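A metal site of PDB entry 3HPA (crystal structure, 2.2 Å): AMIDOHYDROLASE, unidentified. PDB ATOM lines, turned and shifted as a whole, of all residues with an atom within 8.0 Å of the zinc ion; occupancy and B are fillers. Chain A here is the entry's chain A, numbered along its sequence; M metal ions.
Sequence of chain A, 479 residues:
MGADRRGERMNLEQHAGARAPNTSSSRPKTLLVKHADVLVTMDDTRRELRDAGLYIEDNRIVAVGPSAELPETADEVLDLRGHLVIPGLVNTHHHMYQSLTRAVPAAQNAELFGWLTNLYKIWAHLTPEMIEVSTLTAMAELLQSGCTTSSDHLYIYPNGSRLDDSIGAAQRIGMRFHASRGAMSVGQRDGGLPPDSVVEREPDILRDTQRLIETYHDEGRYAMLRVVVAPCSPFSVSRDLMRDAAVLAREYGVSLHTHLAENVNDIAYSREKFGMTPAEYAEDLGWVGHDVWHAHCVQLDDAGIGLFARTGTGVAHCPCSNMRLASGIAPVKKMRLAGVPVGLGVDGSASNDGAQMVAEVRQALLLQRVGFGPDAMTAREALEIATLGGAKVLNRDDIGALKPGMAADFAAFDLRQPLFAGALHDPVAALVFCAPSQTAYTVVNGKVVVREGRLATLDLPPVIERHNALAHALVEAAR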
ATOM      1  N   HIS A  93     -10.902 -21.349  12.048  1.00  0.00           N
ATOM      2  CA  HIS A  93     -12.335 -21.621  12.018  1.00  0.00           C
ATOM      3  C   HIS A  93     -13.113 -20.321  12.132  1.00  0.00           C
ATOM      4  O   HIS A  93     -12.820 -19.498  12.995  1.00  0.00           O
ATOM      5  CB  HIS A  93     -12.790 -22.587  13.108  1.00  0.00           C
ATOM      6  CG  HIS A  93     -14.180 -23.091  12.910  1.00  0.00           C
ATOM      7  ND1 HIS A  93     -14.583 -23.725  11.749  1.00  0.00           N
ATOM      8  CD2 HIS A  93     -15.274 -23.043  13.707  1.00  0.00           C
ATOM      9  CE1 HIS A  93     -15.858 -24.052  11.852  1.00  0.00           C
ATOM     10  NE2 HIS A  93     -16.306 -23.652  13.024  1.00  0.00           N
ATOM     11  N   HIS A  94     -14.116 -20.169  11.259  1.00  0.00           N
ATOM     12  CA  HIS A  94     -14.926 -18.950  11.235  1.00  0.00           C
ATOM     13  C   HIS A  94     -16.229 -19.152  10.449  1.00  0.00           C
ATOM     14  O   HIS A  94     -16.401 -20.135   9.717  1.00  0.00           O
ATOM     15  CB  HIS A  94     -14.126 -17.828  10.542  1.00  0.00           C
ATOM     16  CG  HIS A  94     -14.414 -16.460  11.070  1.00  0.00           C
ATOM     17  ND1 HIS A  94     -15.680 -16.025  11.389  1.00  0.00           N
ATOM     18  CD2 HIS A  94     -13.577 -15.428  11.352  1.00  0.00           C
ATOM     19  CE1 HIS A  94     -15.611 -14.785  11.852  1.00  0.00           C
ATOM     20  NE2 HIS A  94     -14.352 -14.406  11.843  1.00  0.00           N
ATOM     21  N   HIS A  95     -17.136 -18.201  10.612  1.00  0.00           N
ATOM     22  CA  HIS A  95     -18.419 -18.117   9.903  1.00  0.00           C
ATOM     23  C   HIS A  95     -18.528 -16.592   9.762  1.00  0.00           C
ATOM     24  O   HIS A  95     -19.314 -15.930  10.451  1.00  0.00           O
ATOM     25  CB  HIS A  95     -19.567 -18.693  10.728  1.00  0.00           C
ATOM     26  CG  HIS A  95     -19.420 -20.156  11.010  1.00  0.00           C
ATOM     27  ND1 HIS A  95     -19.313 -21.097  10.007  1.00  0.00           N
ATOM     28  CD2 HIS A  95     -19.319 -20.837  12.175  1.00  0.00           C
ATOM     29  CE1 HIS A  95     -19.159 -22.291  10.551  1.00  0.00           C
ATOM     30  NE2 HIS A  95     -19.159 -22.165  11.858  1.00  0.00           N
ATOM     31  N   GLN A  98     -21.587 -14.303   9.746  1.00  0.00           N
ATOM     32  CA  GLN A  98     -22.267 -14.062  11.013  1.00  0.00           C
ATOM     33  C   GLN A  98     -21.922 -12.718  11.641  1.00  0.00           C
ATOM     34  O   GLN A  98     -22.567 -12.294  12.604  1.00  0.00           O
ATOM     35  CB  GLN A  98     -21.997 -15.205  11.999  1.00  0.00           C
ATOM     36  CG  GLN A  98     -22.840 -16.452  11.762  1.00  0.00           C
ATOM     37  CD  GLN A  98     -22.451 -17.609  12.654  1.00  0.00           C
ATOM     38  OE1 GLN A  98     -21.996 -17.415  13.780  1.00  0.00           O
ATOM     39  NE2 GLN A  98     -22.639 -18.833  12.153  1.00  0.00           N
ATOM     40  N   TRP A 115     -30.697 -20.879  19.519  1.00  0.00           N
ATOM     41  CA  TRP A 115     -29.707 -20.015  18.878  1.00  0.00           C
ATOM     42  C   TRP A 115     -29.866 -20.230  17.378  1.00  0.00           C
ATOM     43  O   TRP A 115     -29.952 -19.272  16.595  1.00  0.00           O
ATOM     44  CB  TRP A 115     -28.318 -20.454  19.324  1.00  0.00           C
ATOM     45  CG  TRP A 115     -27.168 -19.597  18.860  1.00  0.00           C
ATOM     46  CD1 TRP A 115     -26.680 -18.471  19.455  1.00  0.00           C
ATOM     47  CD2 TRP A 115     -26.332 -19.843  17.719  1.00  0.00           C
ATOM     48  NE1 TRP A 115     -25.578 -18.001  18.770  1.00  0.00           N
ATOM     49  CE2 TRP A 115     -25.341 -18.825  17.702  1.00  0.00           C
ATOM     50  CE3 TRP A 115     -26.319 -20.828  16.717  1.00  0.00           C
ATOM     51  CZ2 TRP A 115     -24.348 -18.771  16.711  1.00  0.00           C
ATOM     52  CZ3 TRP A 115     -25.328 -20.761  15.744  1.00  0.00           C
ATOM     53  CH2 TRP A 115     -24.355 -19.745  15.748  1.00  0.00           C
ATOM     54  N   HIS A 153     -15.931 -20.756   6.979  1.00  0.00           N
ATOM     55  CA  HIS A 153     -16.799 -21.913   6.829  1.00  0.00           C
ATOM     56  C   HIS A 153     -18.213 -21.449   6.522  1.00  0.00           C
ATOM     57  O   HIS A 153     -19.087 -21.482   7.384  1.00  0.00           O
ATOM     58  CB  HIS A 153     -16.747 -22.732   8.129  1.00  0.00           C
ATOM     59  CG  HIS A 153     -17.434 -24.064   8.040  1.00  0.00           C
ATOM     60  ND1 HIS A 153     -17.674 -24.704   6.843  1.00  0.00           N
ATOM     61  CD2 HIS A 153     -17.904 -24.885   9.007  1.00  0.00           C
ATOM     62  CE1 HIS A 153     -18.262 -25.869   7.078  1.00  0.00           C
ATOM     63  NE2 HIS A 153     -18.417 -26.001   8.381  1.00  0.00           N
ATOM     64  N   TYR A 155     -21.411 -22.267   5.070  1.00  0.00           N
ATOM     65  CA  TYR A 155     -22.171 -23.466   4.730  1.00  0.00           C
ATOM     66  C   TYR A 155     -23.581 -23.219   4.213  1.00  0.00           C
ATOM     67  O   TYR A 155     -24.348 -24.169   4.018  1.00  0.00           O
ATOM     68  CB  TYR A 155     -22.221 -24.408   5.932  1.00  0.00           C
ATOM     69  CG  TYR A 155     -22.869 -23.798   7.170  1.00  0.00           C
ATOM     70  CD1 TYR A 155     -24.254 -23.782   7.316  1.00  0.00           C
ATOM     71  CD2 TYR A 155     -22.084 -23.218   8.162  1.00  0.00           C
ATOM     72  CE1 TYR A 155     -24.848 -23.177   8.432  1.00  0.00           C
ATOM     73  CE2 TYR A 155     -22.669 -22.610   9.277  1.00  0.00           C
ATOM     74  CZ  TYR A 155     -24.054 -22.596   9.413  1.00  0.00           C
ATOM     75  OH  TYR A 155     -24.635 -21.971  10.495  1.00  0.00           O
ATOM     76  N   CYS A 232     -20.896 -28.857   6.557  1.00  0.00           N
ATOM     77  CA  CYS A 232     -21.078 -28.382   7.929  1.00  0.00           C
ATOM     78  C   CYS A 232     -20.735 -29.408   9.016  1.00  0.00           C
ATOM     79  O   CYS A 232     -20.100 -29.062  10.020  1.00  0.00           O
ATOM     80  CB  CYS A 232     -22.513 -27.882   8.123  1.00  0.00           C
ATOM     81  SG  CYS A 232     -22.779 -26.954   9.672  1.00  0.00           S
ATOM     82  N   HIS A 257     -12.698 -30.184   6.009  1.00  0.00           N
ATOM     83  CA  HIS A 257     -12.989 -29.541   7.288  1.00  0.00           C
ATOM     84  C   HIS A 257     -14.462 -29.654   7.630  1.00  0.00           C
ATOM     85  O   HIS A 257     -15.329 -29.593   6.755  1.00  0.00           O
ATOM     86  CB  HIS A 257     -12.586 -28.063   7.225  1.00  0.00           C
ATOM     87  CG  HIS A 257     -12.789 -27.315   8.504  1.00  0.00           C
ATOM     88  ND1 HIS A 257     -13.519 -26.145   8.576  1.00  0.00           N
ATOM     89  CD2 HIS A 257     -12.291 -27.519   9.751  1.00  0.00           C
ATOM     90  CE1 HIS A 257     -13.466 -25.662   9.805  1.00  0.00           C
ATOM     91  NE2 HIS A 257     -12.728 -26.474  10.539  1.00  0.00           N
ATOM     92  N   THR A 258     -14.748 -29.799   8.920  1.00  0.00           N
ATOM     93  CA  THR A 258     -16.133 -29.895   9.377  1.00  0.00           C
ATOM     94  C   THR A 258     -16.212 -29.758  10.889  1.00  0.00           C
ATOM     95  O   THR A 258     -15.182 -29.703  11.567  1.00  0.00           O
ATOM     96  CB  THR A 258     -16.737 -31.250   8.974  1.00  0.00           C
ATOM     97  OG1 THR A 258     -18.137 -31.246   9.285  1.00  0.00           O
ATOM     98  CG2 THR A 258     -16.054 -32.385   9.730  1.00  0.00           C
ATOM     99  N   HIS A 259     -17.434 -29.698  11.416  1.00  0.00           N
ATOM    100  CA  HIS A 259     -17.639 -29.614  12.860  1.00  0.00           C
ATOM    101  C   HIS A 259     -17.634 -31.043  13.405  1.00  0.00           C
ATOM    102  O   HIS A 259     -18.145 -31.963  12.759  1.00  0.00           O
ATOM    103  CB  HIS A 259     -19.004 -28.985  13.173  1.00  0.00           C
ATOM    104  CG  HIS A 259     -19.114 -27.537  12.791  1.00  0.00           C
ATOM    105  ND1 HIS A 259     -19.807 -27.124  11.672  1.00  0.00           N
ATOM    106  CD2 HIS A 259     -18.646 -26.418  13.378  1.00  0.00           C
ATOM    107  CE1 HIS A 259     -19.759 -25.801  11.596  1.00  0.00           C
ATOM    108  NE2 HIS A 259     -19.065 -25.352  12.622  1.00  0.00           N
ATOM    109  N   GLU A 262     -18.753 -31.323  19.177  1.00  0.00           N
ATOM    110  CA  GLU A 262     -18.809 -30.048  19.883  1.00  0.00           C
ATOM    111  C   GLU A 262     -19.636 -30.009  21.157  1.00  0.00           C
ATOM    112  O   GLU A 262     -19.423 -29.154  22.018  1.00  0.00           O
ATOM    113  CB  GLU A 262     -19.274 -28.937  18.940  1.00  0.00           C
ATOM    114  CG  GLU A 262     -20.158 -29.407  17.803  1.00  0.00           C
ATOM    115  CD  GLU A 262     -20.613 -28.277  16.907  1.00  0.00           C
ATOM    116  OE1 GLU A 262     -21.163 -28.572  15.831  1.00  0.00           O
ATOM    117  OE2 GLU A 262     -20.434 -27.093  17.294  1.00  0.00           O
ATOM    118  N   ALA A 295     -13.312 -28.711  13.726  1.00  0.00           N
ATOM    119  CA  ALA A 295     -13.534 -27.611  14.658  1.00  0.00           C
ATOM    120  C   ALA A 295     -14.223 -28.056  15.951  1.00  0.00           C
ATOM    121  O   ALA A 295     -15.083 -28.939  15.951  1.00  0.00           O
ATOM    122  CB  ALA A 295     -14.366 -26.511  13.995  1.00  0.00           C
ATOM    123  N   HIS A 296     -13.824 -27.421  17.051  1.00  0.00           N
ATOM    124  CA  HIS A 296     -14.372 -27.669  18.378  1.00  0.00           C
ATOM    125  C   HIS A 296     -13.812 -28.918  19.065  1.00  0.00           C
ATOM    126  O   HIS A 296     -12.864 -28.826  19.852  1.00  0.00           O
ATOM    127  CB  HIS A 296     -15.890 -27.728  18.308  1.00  0.00           C
ATOM    128  CG  HIS A 296     -16.513 -26.456  17.823  1.00  0.00           C
ATOM    129  ND1 HIS A 296     -16.189 -25.225  18.358  1.00  0.00           N
ATOM    130  CD2 HIS A 296     -17.448 -26.225  16.873  1.00  0.00           C
ATOM    131  CE1 HIS A 296     -16.904 -24.294  17.757  1.00  0.00           C
ATOM    132  NE2 HIS A 296     -17.673 -24.870  16.845  1.00  0.00           N
ATOM    133  N   CYS A 318     -11.702 -23.348  19.633  1.00  0.00           N
ATOM    134  CA  CYS A 318     -12.397 -22.065  19.706  1.00  0.00           C
ATOM    135  C   CYS A 318     -12.853 -21.847  21.139  1.00  0.00           C
ATOM    136  O   CYS A 318     -14.013 -22.100  21.480  1.00  0.00           O
ATOM    137  CB  CYS A 318     -13.621 -22.037  18.790  1.00  0.00           C
ATOM    138  SG  CYS A 318     -13.255 -22.523  17.098  1.00  0.00           S
ATOM    139  N   SER A 321     -16.002 -19.129  21.800  1.00  0.00           N
ATOM    140  CA  SER A 321     -17.248 -19.718  21.335  1.00  0.00           C
ATOM    141  C   SER A 321     -17.679 -20.835  22.286  1.00  0.00           C
ATOM    142  O   SER A 321     -18.837 -20.899  22.708  1.00  0.00           O
ATOM    143  CB  SER A 321     -17.074 -20.265  19.914  1.00  0.00           C
ATOM    144  OG  SER A 321     -18.266 -20.862  19.448  1.00  0.00           O
ATOM    145  N   VAL A 346     -11.549 -18.339  15.912  1.00  0.00           N
ATOM    146  CA  VAL A 346     -12.389 -17.370  16.587  1.00  0.00           C
ATOM    147  C   VAL A 346     -13.841 -17.847  16.468  1.00  0.00           C
ATOM    148  O   VAL A 346     -14.677 -17.569  17.320  1.00  0.00           O
ATOM    149  CB  VAL A 346     -12.174 -15.938  15.961  1.00  0.00           C
ATOM    150  CG1 VAL A 346     -12.821 -15.842  14.585  1.00  0.00           C
ATOM    151  CG2 VAL A 346     -12.698 -14.875  16.881  1.00  0.00           C
ATOM    152  N   ASP A 347     -14.110 -18.619  15.414  1.00  0.00           N
ATOM    153  CA  ASP A 347     -15.451 -19.147  15.105  1.00  0.00           C
ATOM    154  C   ASP A 347     -16.350 -18.018  14.613  1.00  0.00           C
ATOM    155  O   ASP A 347     -15.925 -16.851  14.526  1.00  0.00           O
ATOM    156  CB  ASP A 347     -16.077 -19.835  16.332  1.00  0.00           C
ATOM    157  CG  ASP A 347     -17.186 -20.837  15.946  1.00  0.00           C
ATOM    158  OD1 ASP A 347     -17.327 -21.160  14.746  1.00  0.00           O
ATOM    159  OD2 ASP A 347     -17.908 -21.316  16.840  1.00  0.00           O
ATOM    160  N   GLY A 348     -17.591 -18.368  14.283  1.00  0.00           N
ATOM    161  CA  GLY A 348     -18.563 -17.403  13.789  1.00  0.00           C
ATOM    162  C   GLY A 348     -18.871 -16.279  14.751  1.00  0.00           C
ATOM    163  O   GLY A 348     -18.994 -16.490  15.954  1.00  0.00           O
ATOM    164  N   SER A 351     -21.402 -16.374  17.565  1.00  0.00           N
ATOM    165  CA  SER A 351     -21.073 -17.140  18.753  1.00  0.00           C
ATOM    166  C   SER A 351     -19.662 -16.837  19.256  1.00  0.00           C
ATOM    167  O   SER A 351     -18.776 -17.700  19.232  1.00  0.00           O
ATOM    168  CB  SER A 351     -21.224 -18.652  18.498  1.00  0.00           C
ATOM    169  OG  SER A 351     -20.240 -19.138  17.601  1.00  0.00           O
HETATM  170 ZN    ZN M   1     -18.362 -23.325  13.463  1.00  0.00          ZN
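The zinc ion is bound by a ring nitrogen (NE2) of His 93 (2.1 Å), a ring nitrogen (NE2) of His 95 (2.1 Å) and a ring nitrogen (NE2) of His 259 (2.3 Å). Slightly farther from the zinc ion lies the side-chain carboxylate (OD1) of Asp 347 (2.7 Å).
O of His 93 lies within hydrogen-bond range of N of Asp 347 (2.9 Å). O of His 93 lies within hydrogen-bond range of N of Val 346 (3.4 Å). A ring nitrogen (ND1) of His 95 lies within hydrogen-bond range of the backbone carbonyl oxygen (O) of His 153. A ring nitrogen (ND1) of His 259 is in hydrogen-bond range of the backbone carbonyl oxygen (O) of Cys 232, at 2.6 Å. O of Asp 347 sits at hydrogen-bond distance from ND1 of His 94 (3.3 Å). The side-chain hydroxyl (OG) of Ser 351 is in hydrogen-bond range of the side-chain carboxylate (OD2) of Asp 347, at 3.3 Å. The side-chain carboxylate (OD2) of Asp 347 lies within hydrogen-bond range of the side-chain hydroxyl (OG) of Ser 321, at 2.7 Å.
NE2 of His 296 touches the zinc ion, at 3.8 Å. Five residues have an atom within 4 Å of the zinc ion: His 93, His 95, His 259, His 296 and Asp 347. Along chain A the residues within 4 Å of the zinc ion span positions 93 to 347. The nearest printed residue that does not touch the zinc ion is His 153 (4.7 Å).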
